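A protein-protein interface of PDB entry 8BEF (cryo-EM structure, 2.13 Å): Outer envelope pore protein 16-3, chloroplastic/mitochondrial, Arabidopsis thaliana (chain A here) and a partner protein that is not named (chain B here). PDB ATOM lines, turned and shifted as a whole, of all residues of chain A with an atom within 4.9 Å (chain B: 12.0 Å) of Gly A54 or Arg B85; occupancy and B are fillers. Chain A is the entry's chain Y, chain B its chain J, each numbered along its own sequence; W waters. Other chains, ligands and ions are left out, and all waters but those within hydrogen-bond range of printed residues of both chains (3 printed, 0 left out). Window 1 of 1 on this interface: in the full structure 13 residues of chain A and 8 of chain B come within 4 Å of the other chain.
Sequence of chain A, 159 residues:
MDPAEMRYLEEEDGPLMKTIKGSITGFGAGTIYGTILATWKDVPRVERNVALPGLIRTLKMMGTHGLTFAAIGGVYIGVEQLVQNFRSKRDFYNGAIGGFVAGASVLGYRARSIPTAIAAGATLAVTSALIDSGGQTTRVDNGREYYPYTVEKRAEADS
OG1 of Thr A58 sits at hydrogen-bond distance from O of Gly A54, 3.3 Å away. OH of Tyr B86 is in hydrogen-bond range of OE2 of Glu B81 (2.8 Å). The guanidinium group (NH1) of Arg B85 is in hydrogen-bond range of the side-chain hydroxyl (OH) of Tyr B86 (2.9 Å). The backbone carbonyl oxygen (O) of Tyr B86 lies within hydrogen-bond range of the side-chain hydroxyl (OG) of Ser B90 (3.1 Å).
Ala A38 touches just one residue of chain B: Arg B85 (2.6 Å). Printed residues of chain B within 4 Å of Lys A41: Arg B85 (2.9 Å). No residue of chain B comes within 4 Å of Asp A42. Val A43 touches just one residue of chain B: Arg B85 (3.7 Å). Ala A51 touches just these residues of chain B: Glu B82 (3.3 Å) and Leu B84 (3.8 Å). Leu A52 touches none of the printed residues of chain B. No residue of chain B comes within 4 Å of Pro A53. Gly A54 touches just one residue of chain B: Arg B85. No residue of chain B comes within 4 Å of Ile A56. No residue of chain B comes within 4 Å of Arg A57. Printed residues of chain B within 4 Å of Thr A58: Arg B85 and Pro B88. Of the printed residues of chain A, Glu B82 touches Ala A51. Arg B85 touches just these residues of chain A: Ala A38 (2.6 Å), Thr A39 (3.8 Å), Lys A41 (2.9 Å), Val A43 (3.7 Å), Gly A54 (3.7 Å), Leu A55 (3.7 Å) and Thr A58 (3.9 Å). Of the printed residues of chain A, Val B89 touches Thr A39 (3.5 Å). The nearest residue of chain B that does not touch Gly A54 is Leu B84 (5.9 Å).
CD1 of Tyr B86 touches CG2 of Thr A39, 3.7 Å away. Thr A39 touches Val B89. Val A43 touches Arg B85 (CG1 to CD, 3.7 Å). Ala A51 touches Glu B82 (CB to OE1, 3.3 Å). Leu B84 touches Ala A51. Gly A54 touches Arg B85 (C to CB, 3.7 Å). Leu A55 touches Leu B84 (CD1 to O, 3.4 Å). Leu A55 touches Arg B85 (N to CB, 3.7 Å). Thr A58 touches Arg B85. Pro B88 touches Thr A58.
O of Ala A38 is in hydrogen-bond range of NH2 of Arg B85, 2.6 Å away. O of Lys A41 lies within hydrogen-bond range of NH2 of Arg B85 (2.9 Å).
Water W2 lies within hydrogen-bond range of N of Arg B85, N of Leu B84 and O of Ala A51. Water W3 lies within hydrogen-bond range of O of Arg B85 (2.6 Å), N of Val B89 (3.1 Å) and OG1 of Thr A39 (3.2 Å). Water W1 lies within hydrogen-bond range of O of Arg B85 (2.8 Å), OG1 of Thr A58 (2.9 Å) and OG1 of Thr A39 (3.2 Å).
Printed residues of chain B that touch a printed residue of chain A: Glu B82, Leu B84, Arg B85, Tyr B86, Pro B88 and Val B89. Of the 14 printed residues of chain A, 8 touch a printed residue of chain B. Printed residues of chain A that touch a printed residue of chain B: Ala A38, Thr A39, Lys A41, Val A43, Ala A51, Gly A54, Leu A55 and Thr A58. Hydrophobic or aromatic side chains of chain A within 4 Å of the printed part of chain B: Val A43, Ala A51 and Leu A55. Among the printed residues, 13 pairs touch across the chains. Among the printed residues, no Asp or Glu carboxylate lies within 4 Å of a Lys or Arg side-chain nitrogen of the other chain.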
ATOM      1  N   ALA A  38       8.734  14.812  17.203  1.00  0.00           N
ATOM      2  CA  ALA A  38       9.427  16.090  17.109  1.00  0.00           C
ATOM      3  C   ALA A  38       8.445  17.253  17.130  1.00  0.00           C
ATOM      4  O   ALA A  38       8.697  18.275  17.775  1.00  0.00           O
ATOM      5  CB  ALA A  38      10.284  16.126  15.844  1.00  0.00           C
ATOM      6  N   THR A  39       7.319  17.159  16.473  1.00  0.00           N
ATOM      7  CA  THR A  39       6.321  18.259  16.440  1.00  0.00           C
ATOM      8  C   THR A  39       5.647  18.428  17.834  1.00  0.00           C
ATOM      9  O   THR A  39       5.373  19.523  18.196  1.00  0.00           O
ATOM     10  CB  THR A  39       5.334  18.013  15.299  1.00  0.00           C
ATOM     11  OG1 THR A  39       6.036  17.631  14.117  1.00  0.00           O
ATOM     12  CG2 THR A  39       4.440  19.200  15.018  1.00  0.00           C
ATOM     13  N   LYS A  41       6.883  18.063  20.876  1.00  0.00           N
ATOM     14  CA  LYS A  41       7.760  18.751  21.860  1.00  0.00           C
ATOM     15  C   LYS A  41       7.956  20.231  21.583  1.00  0.00           C
ATOM     16  O   LYS A  41       7.829  20.673  20.444  1.00  0.00           O
ATOM     17  CB  LYS A  41       9.137  18.091  21.929  1.00  0.00           C
ATOM     18  CG  LYS A  41       9.099  16.594  21.708  1.00  0.00           C
ATOM     19  CD  LYS A  41      10.436  16.029  21.300  1.00  0.00           C
ATOM     20  CE  LYS A  41      11.431  16.042  22.437  1.00  0.00           C
ATOM     21  NZ  LYS A  41      10.887  15.352  23.627  1.00  0.00           N
ATOM     22  N   ASP A  42       8.389  20.913  22.621  1.00  0.00           N
ATOM     23  CA  ASP A  42       8.658  22.369  22.535  1.00  0.00           C
ATOM     24  C   ASP A  42      10.075  22.531  22.010  1.00  0.00           C
ATOM     25  O   ASP A  42      10.778  21.507  21.957  1.00  0.00           O
ATOM     26  CB  ASP A  42       8.528  22.992  23.919  1.00  0.00           C
ATOM     27  CG  ASP A  42       9.655  22.575  24.839  1.00  0.00           C
ATOM     28  OD1 ASP A  42       9.677  21.395  25.234  1.00  0.00           O
ATOM     29  OD2 ASP A  42      10.517  23.427  25.124  1.00  0.00           O
ATOM     30  N   VAL A  43      10.456  23.731  21.617  1.00  0.00           N
ATOM     31  CA  VAL A  43      11.838  24.012  21.238  1.00  0.00           C
ATOM     32  C   VAL A  43      12.580  24.547  22.457  1.00  0.00           C
ATOM     33  O   VAL A  43      11.969  25.192  23.319  1.00  0.00           O
ATOM     34  CB  VAL A  43      11.914  25.006  20.069  1.00  0.00           C
ATOM     35  CG1 VAL A  43      11.731  24.280  18.742  1.00  0.00           C
ATOM     36  CG2 VAL A  43      10.878  26.103  20.237  1.00  0.00           C
ATOM     37  N   GLU A  47      16.622  28.498  21.379  1.00  0.00           N
ATOM     38  CA  GLU A  47      16.379  28.247  19.963  1.00  0.00           C
ATOM     39  C   GLU A  47      15.069  28.867  19.492  1.00  0.00           C
ATOM     40  O   GLU A  47      14.584  28.532  18.408  1.00  0.00           O
ATOM     41  CB  GLU A  47      16.386  26.744  19.682  1.00  0.00           C
ATOM     42  CG  GLU A  47      17.712  26.082  19.993  1.00  0.00           C
ATOM     43  CD  GLU A  47      17.874  24.751  19.297  1.00  0.00           C
ATOM     44  OE1 GLU A  47      18.446  23.827  19.910  1.00  0.00           O
ATOM     45  OE2 GLU A  47      17.413  24.622  18.146  1.00  0.00           O
ATOM     46  N   ALA A  51      15.526  29.402  13.376  1.00  0.00           N
ATOM     47  CA  ALA A  51      14.677  28.392  12.755  1.00  0.00           C
ATOM     48  C   ALA A  51      15.418  27.107  12.400  1.00  0.00           C
ATOM     49  O   ALA A  51      14.890  26.013  12.626  1.00  0.00           O
ATOM     50  CB  ALA A  51      14.025  28.963  11.496  1.00  0.00           C
ATOM     51  N   LEU A  52      16.620  27.220  11.831  1.00  0.00           N
ATOM     52  CA  LEU A  52      17.276  26.059  11.229  1.00  0.00           C
ATOM     53  C   LEU A  52      17.517  24.913  12.207  1.00  0.00           C
ATOM     54  O   LEU A  52      17.167  23.769  11.869  1.00  0.00           O
ATOM     55  CB  LEU A  52      18.582  26.503  10.557  1.00  0.00           C
ATOM     56  CG  LEU A  52      19.362  25.472   9.732  1.00  0.00           C
ATOM     57  CD1 LEU A  52      18.438  24.539   8.964  1.00  0.00           C
ATOM     58  CD2 LEU A  52      20.328  26.167   8.784  1.00  0.00           C
ATOM     59  N   PRO A  53      18.095  25.120  13.397  1.00  0.00           N
ATOM     60  CA  PRO A  53      18.375  23.964  14.271  1.00  0.00           C
ATOM     61  C   PRO A  53      17.139  23.189  14.687  1.00  0.00           C
ATOM     62  O   PRO A  53      17.243  21.985  14.937  1.00  0.00           O
ATOM     63  CB  PRO A  53      19.072  24.595  15.484  1.00  0.00           C
ATOM     64  CG  PRO A  53      18.723  26.020  15.426  1.00  0.00           C
ATOM     65  CD  PRO A  53      18.630  26.362  13.983  1.00  0.00           C
ATOM     66  N   GLY A  54      15.975  23.835  14.789  1.00  0.00           N
ATOM     67  CA  GLY A  54      14.759  23.088  15.069  1.00  0.00           C
ATOM     68  C   GLY A  54      14.418  22.113  13.961  1.00  0.00           C
ATOM     69  O   GLY A  54      14.088  20.951  14.217  1.00  0.00           O
ATOM     70  N   LEU A  55      14.518  22.566  12.710  1.00  0.00           N
ATOM     71  CA  LEU A  55      14.339  21.670  11.575  1.00  0.00           C
ATOM     72  C   LEU A  55      15.383  20.561  11.587  1.00  0.00           C
ATOM     73  O   LEU A  55      15.069  19.399  11.301  1.00  0.00           O
ATOM     74  CB  LEU A  55      14.411  22.464  10.271  1.00  0.00           C
ATOM     75  CG  LEU A  55      14.448  21.659   8.973  1.00  0.00           C
ATOM     76  CD1 LEU A  55      13.047  21.234   8.566  1.00  0.00           C
ATOM     77  CD2 LEU A  55      15.107  22.463   7.871  1.00  0.00           C
ATOM     78  N   ILE A  56      16.629  20.902  11.922  1.00  0.00           N
ATOM     79  CA  ILE A  56      17.694  19.902  11.957  1.00  0.00           C
ATOM     80  C   ILE A  56      17.391  18.836  13.003  1.00  0.00           C
ATOM     81  O   ILE A  56      17.547  17.637  12.755  1.00  0.00           O
ATOM     82  CB  ILE A  56      19.056  20.573  12.219  1.00  0.00           C
ATOM     83  CG1 ILE A  56      19.422  21.519  11.072  1.00  0.00           C
ATOM     84  CG2 ILE A  56      20.133  19.525  12.404  1.00  0.00           C
ATOM     85  CD1 ILE A  56      19.231  20.922   9.704  1.00  0.00           C
ATOM     86  N   ARG A  57      16.962  19.260  14.193  1.00  0.00           N
ATOM     87  CA  ARG A  57      16.637  18.309  15.250  1.00  0.00           C
ATOM     88  C   ARG A  57      15.445  17.441  14.869  1.00  0.00           C
ATOM     89  O   ARG A  57      15.432  16.236  15.150  1.00  0.00           O
ATOM     90  CB  ARG A  57      16.380  19.051  16.565  1.00  0.00           C
ATOM     91  CG  ARG A  57      15.405  18.350  17.493  1.00  0.00           C
ATOM     92  CD  ARG A  57      14.913  19.219  18.654  1.00  0.00           C
ATOM     93  NE  ARG A  57      15.970  19.990  19.302  1.00  0.00           N
ATOM     94  CZ  ARG A  57      16.336  21.219  18.968  1.00  0.00           C
ATOM     95  NH1 ARG A  57      15.725  21.886  18.004  1.00  0.00           N
ATOM     96  NH2 ARG A  57      17.340  21.794  19.623  1.00  0.00           N
ATOM     97  N   THR A  58      14.440  18.032  14.219  1.00  0.00           N
ATOM     98  CA  THR A  58      13.297  17.247  13.763  1.00  0.00           C
ATOM     99  C   THR A  58      13.727  16.189  12.753  1.00  0.00           C
ATOM    100  O   THR A  58      13.313  15.028  12.838  1.00  0.00           O
ATOM    101  CB  THR A  58      12.236  18.170  13.159  1.00  0.00           C
ATOM    102  OG1 THR A  58      11.559  18.873  14.206  1.00  0.00           O
ATOM    103  CG2 THR A  58      11.220  17.369  12.360  1.00  0.00           C
ATOM    104  N   ARG B  19      -0.032  32.822   7.858  1.00  0.00           N
ATOM    105  CA  ARG B  19       1.401  33.011   8.043  1.00  0.00           C
ATOM    106  C   ARG B  19       1.836  34.445   8.331  1.00  0.00           C
ATOM    107  O   ARG B  19       3.002  34.649   8.684  1.00  0.00           O
ATOM    108  CB  ARG B  19       2.172  32.505   6.812  1.00  0.00           C
ATOM    109  CG  ARG B  19       2.148  30.993   6.639  1.00  0.00           C
ATOM    110  CD  ARG B  19       3.464  30.357   7.060  1.00  0.00           C
ATOM    111  NE  ARG B  19       3.848  30.696   8.425  1.00  0.00           N
ATOM    112  CZ  ARG B  19       4.857  31.497   8.742  1.00  0.00           C
ATOM    113  NH1 ARG B  19       5.599  32.076   7.812  1.00  0.00           N
ATOM    114  NH2 ARG B  19       5.130  31.720  10.024  1.00  0.00           N
ATOM    115  N   ILE B  79       3.326  35.916  20.247  1.00  0.00           N
ATOM    116  CA  ILE B  79       2.692  34.923  19.342  1.00  0.00           C
ATOM    117  C   ILE B  79       3.722  34.463  18.294  1.00  0.00           C
ATOM    118  O   ILE B  79       3.333  33.751  17.431  1.00  0.00           O
ATOM    119  CB  ILE B  79       1.394  35.550  18.765  1.00  0.00           C
ATOM    120  CG1 ILE B  79       1.745  36.906  18.142  1.00  0.00           C
ATOM    121  CG2 ILE B  79       0.289  35.685  19.786  1.00  0.00           C
ATOM    122  CD1 ILE B  79       0.959  37.288  16.925  1.00  0.00           C
ATOM    123  N   HIS B  80       4.977  34.923  18.372  1.00  0.00           N
ATOM    124  CA  HIS B  80       5.996  34.525  17.413  1.00  0.00           C
ATOM    125  C   HIS B  80       6.457  33.092  17.650  1.00  0.00           C
ATOM    126  O   HIS B  80       6.554  32.628  18.789  1.00  0.00           O
ATOM    127  CB  HIS B  80       7.207  35.452  17.489  1.00  0.00           C
ATOM    128  CG  HIS B  80       8.509  34.753  17.260  1.00  0.00           C
ATOM    129  ND1 HIS B  80       9.044  34.570  16.004  1.00  0.00           N
ATOM    130  CD2 HIS B  80       9.373  34.168  18.124  1.00  0.00           C
ATOM    131  CE1 HIS B  80      10.183  33.911  16.104  1.00  0.00           C
ATOM    132  NE2 HIS B  80      10.406  33.656  17.380  1.00  0.00           N
ATOM    133  N   GLU B  81       6.794  32.473  16.536  1.00  0.00           N
ATOM    134  CA  GLU B  81       7.453  31.141  16.607  1.00  0.00           C
ATOM    135  C   GLU B  81       7.981  30.809  15.207  1.00  0.00           C
ATOM    136  O   GLU B  81       7.297  31.131  14.261  1.00  0.00           O
ATOM    137  CB  GLU B  81       6.550  30.030  17.122  1.00  0.00           C
ATOM    138  CG  GLU B  81       6.887  28.653  16.635  1.00  0.00           C
ATOM    139  CD  GLU B  81       5.838  27.652  17.040  1.00  0.00           C
ATOM    140  OE1 GLU B  81       4.775  27.636  16.414  1.00  0.00           O
ATOM    141  OE2 GLU B  81       6.079  26.937  18.000  1.00  0.00           O
ATOM    142  N   GLU B  82       9.102  30.131  15.131  1.00  0.00           N
ATOM    143  CA  GLU B  82       9.643  29.668  13.858  1.00  0.00           C
ATOM    144  C   GLU B  82       8.859  28.465  13.349  1.00  0.00           C
ATOM    145  O   GLU B  82       8.558  27.542  14.110  1.00  0.00           O
ATOM    146  CB  GLU B  82      11.114  29.300  14.017  1.00  0.00           C
ATOM    147  CG  GLU B  82      11.884  30.245  14.901  1.00  0.00           C
ATOM    148  CD  GLU B  82      12.412  31.435  14.139  1.00  0.00           C
ATOM    149  OE1 GLU B  82      12.385  31.400  12.891  1.00  0.00           O
ATOM    150  OE2 GLU B  82      12.848  32.410  14.784  1.00  0.00           O
ATOM    151  N   VAL B  83       8.545  28.466  12.055  1.00  0.00           N
ATOM    152  CA  VAL B  83       7.742  27.411  11.450  1.00  0.00           C
ATOM    153  C   VAL B  83       8.547  26.511  10.527  1.00  0.00           C
ATOM    154  O   VAL B  83       7.964  25.617   9.900  1.00  0.00           O
ATOM    155  CB  VAL B  83       6.529  27.987  10.697  1.00  0.00           C
ATOM    156  CG1 VAL B  83       5.623  28.752  11.650  1.00  0.00           C
ATOM    157  CG2 VAL B  83       6.989  28.869   9.554  1.00  0.00           C
ATOM    158  N   LEU B  84       9.864  26.714  10.418  1.00  0.00           N
ATOM    159  CA  LEU B  84      10.673  25.845   9.567  1.00  0.00           C
ATOM    160  C   LEU B  84      10.600  24.394  10.024  1.00  0.00           C
ATOM    161  O   LEU B  84      10.582  23.481   9.193  1.00  0.00           O
ATOM    162  CB  LEU B  84      12.124  26.330   9.550  1.00  0.00           C
ATOM    163  CG  LEU B  84      13.121  25.695   8.573  1.00  0.00           C
ATOM    164  CD1 LEU B  84      12.445  25.269   7.289  1.00  0.00           C
ATOM    165  CD2 LEU B  84      14.279  26.639   8.283  1.00  0.00           C
ATOM    166  N   ARG B  85      10.542  24.114  11.316  1.00  0.00           N
ATOM    167  CA  ARG B  85      10.518  22.753  11.893  1.00  0.00           C
ATOM    168  C   ARG B  85       9.142  22.062  11.686  1.00  0.00           C
ATOM    169  O   ARG B  85       9.044  20.931  12.096  1.00  0.00           O
ATOM    170  CB  ARG B  85      10.887  22.854  13.370  1.00  0.00           C
ATOM    171  CG  ARG B  85       9.783  23.566  14.145  1.00  0.00           C
ATOM    172  CD  ARG B  85       9.811  23.701  15.649  1.00  0.00           C
ATOM    173  NE  ARG B  85       9.663  22.420  16.267  1.00  0.00           N
ATOM    174  CZ  ARG B  85       8.919  22.149  17.335  1.00  0.00           C
ATOM    175  NH1 ARG B  85       8.250  23.098  17.956  1.00  0.00           N
ATOM    176  NH2 ARG B  85       8.888  20.915  17.785  1.00  0.00           N
ATOM    177  N   TYR B  86       8.126  22.760  11.207  1.00  0.00           N
ATOM    178  CA  TYR B  86       6.827  22.152  10.867  1.00  0.00           C
ATOM    179  C   TYR B  86       6.749  21.659   9.413  1.00  0.00           C
ATOM    180  O   TYR B  86       5.841  20.899   9.170  1.00  0.00           O
ATOM    181  CB  TYR B  86       5.682  23.077  11.268  1.00  0.00           C
ATOM    182  CG  TYR B  86       5.716  23.432  12.723  1.00  0.00           C
ATOM    183  CD1 TYR B  86       5.385  22.502  13.688  1.00  0.00           C
ATOM    184  CD2 TYR B  86       6.152  24.679  13.128  1.00  0.00           C
ATOM    185  CE1 TYR B  86       5.433  22.821  15.035  1.00  0.00           C
ATOM    186  CE2 TYR B  86       6.214  25.012  14.466  1.00  0.00           C
ATOM    187  CZ  TYR B  86       5.867  24.074  15.420  1.00  0.00           C
ATOM    188  OH  TYR B  86       5.953  24.398  16.729  1.00  0.00           O
ATOM    189  N   LEU B  87       7.674  22.042   8.525  1.00  0.00           N
ATOM    190  CA  LEU B  87       7.592  21.613   7.130  1.00  0.00           C
ATOM    191  C   LEU B  87       7.374  20.113   6.953  1.00  0.00           C
ATOM    192  O   LEU B  87       6.560  19.741   6.091  1.00  0.00           O
ATOM    193  CB  LEU B  87       8.849  22.058   6.366  1.00  0.00           C
ATOM    194  CG  LEU B  87       8.811  23.441   5.718  1.00  0.00           C
ATOM    195  CD1 LEU B  87      10.135  23.752   5.042  1.00  0.00           C
ATOM    196  CD2 LEU B  87       7.666  23.534   4.719  1.00  0.00           C
ATOM    197  N   PRO B  88       8.044  19.213   7.683  1.00  0.00           N
ATOM    198  CA  PRO B  88       7.739  17.782   7.491  1.00  0.00           C
ATOM    199  C   PRO B  88       6.331  17.395   7.917  1.00  0.00           C
ATOM    200  O   PRO B  88       5.613  16.762   7.135  1.00  0.00           O
ATOM    201  CB  PRO B  88       8.817  17.069   8.322  1.00  0.00           C
ATOM    202  CG  PRO B  88       9.812  18.105   8.695  1.00  0.00           C
ATOM    203  CD  PRO B  88       9.138  19.420   8.650  1.00  0.00           C
ATOM    204  N   VAL B  89       5.905  17.767   9.128  1.00  0.00           N
ATOM    205  CA  VAL B  89       4.580  17.362   9.596  1.00  0.00           C
ATOM    206  C   VAL B  89       3.493  17.932   8.694  1.00  0.00           C
ATOM    207  O   VAL B  89       2.477  17.278   8.435  1.00  0.00           O
ATOM    208  CB  VAL B  89       4.370  17.760  11.072  1.00  0.00           C
ATOM    209  CG1 VAL B  89       4.218  19.268  11.232  1.00  0.00           C
ATOM    210  CG2 VAL B  89       3.157  17.047  11.636  1.00  0.00           C
ATOM    211  N   SER B  90       3.684  19.157   8.200  1.00  0.00           N
ATOM    212  CA  SER B  90       2.755  19.698   7.218  1.00  0.00           C
ATOM    213  C   SER B  90       2.875  18.970   5.887  1.00  0.00           C
ATOM    214  O   SER B  90       1.886  18.849   5.156  1.00  0.00           O
ATOM    215  CB  SER B  90       2.997  21.194   7.026  1.00  0.00           C
ATOM    216  OG  SER B  90       4.305  21.434   6.541  1.00  0.00           O
ATOM    217  N   GLY B  91       4.074  18.488   5.556  1.00  0.00           N
ATOM    218  CA  GLY B  91       4.249  17.765   4.308  1.00  0.00           C
ATOM    219  C   GLY B  91       3.476  16.460   4.271  1.00  0.00           C
ATOM    220  O   GLY B  91       2.799  16.159   3.287  1.00  0.00           O
ATOM    221  N   ILE B  92       3.570  15.662   5.337  1.00  0.00           N
ATOM    222  CA  ILE B  92       2.845  14.395   5.366  1.00  0.00           C
ATOM    223  C   ILE B  92       1.345  14.643   5.473  1.00  0.00           C
ATOM    224  O   ILE B  92       0.554  14.084   4.705  1.00  0.00           O
ATOM    225  CB  ILE B  92       3.349  13.497   6.510  1.00  0.00           C
ATOM    226  CG1 ILE B  92       4.858  13.284   6.404  1.00  0.00           C
ATOM    227  CG2 ILE B  92       2.635  12.164   6.485  1.00  0.00           C
ATOM    228  CD1 ILE B  92       5.605  13.589   7.679  1.00  0.00           C
ATOM    229  N   ILE B  93       0.930  15.493   6.413  1.00  0.00           N
ATOM    230  CA  ILE B  93      -0.498  15.731   6.600  1.00  0.00           C
ATOM    231  C   ILE B  93      -1.089  16.391   5.362  1.00  0.00           C
ATOM    232  O   ILE B  93      -2.171  16.016   4.896  1.00  0.00           O
ATOM    233  CB  ILE B  93      -0.749  16.572   7.866  1.00  0.00           C
ATOM    234  CG1 ILE B  93      -0.269  15.828   9.115  1.00  0.00           C
ATOM    235  CG2 ILE B  93      -2.224  16.886   8.000  1.00  0.00           C
ATOM    236  CD1 ILE B  93      -1.127  14.660   9.508  1.00  0.00           C
HETATM  237  O   HOH W   1       8.741  19.387  14.412  1.00  0.00           O
HETATM  238  O   HOH W   2      11.676  25.913  12.745  1.00  0.00           O
HETATM  239  O   HOH W   3       7.478  18.878  11.573  1.00  0.00           O
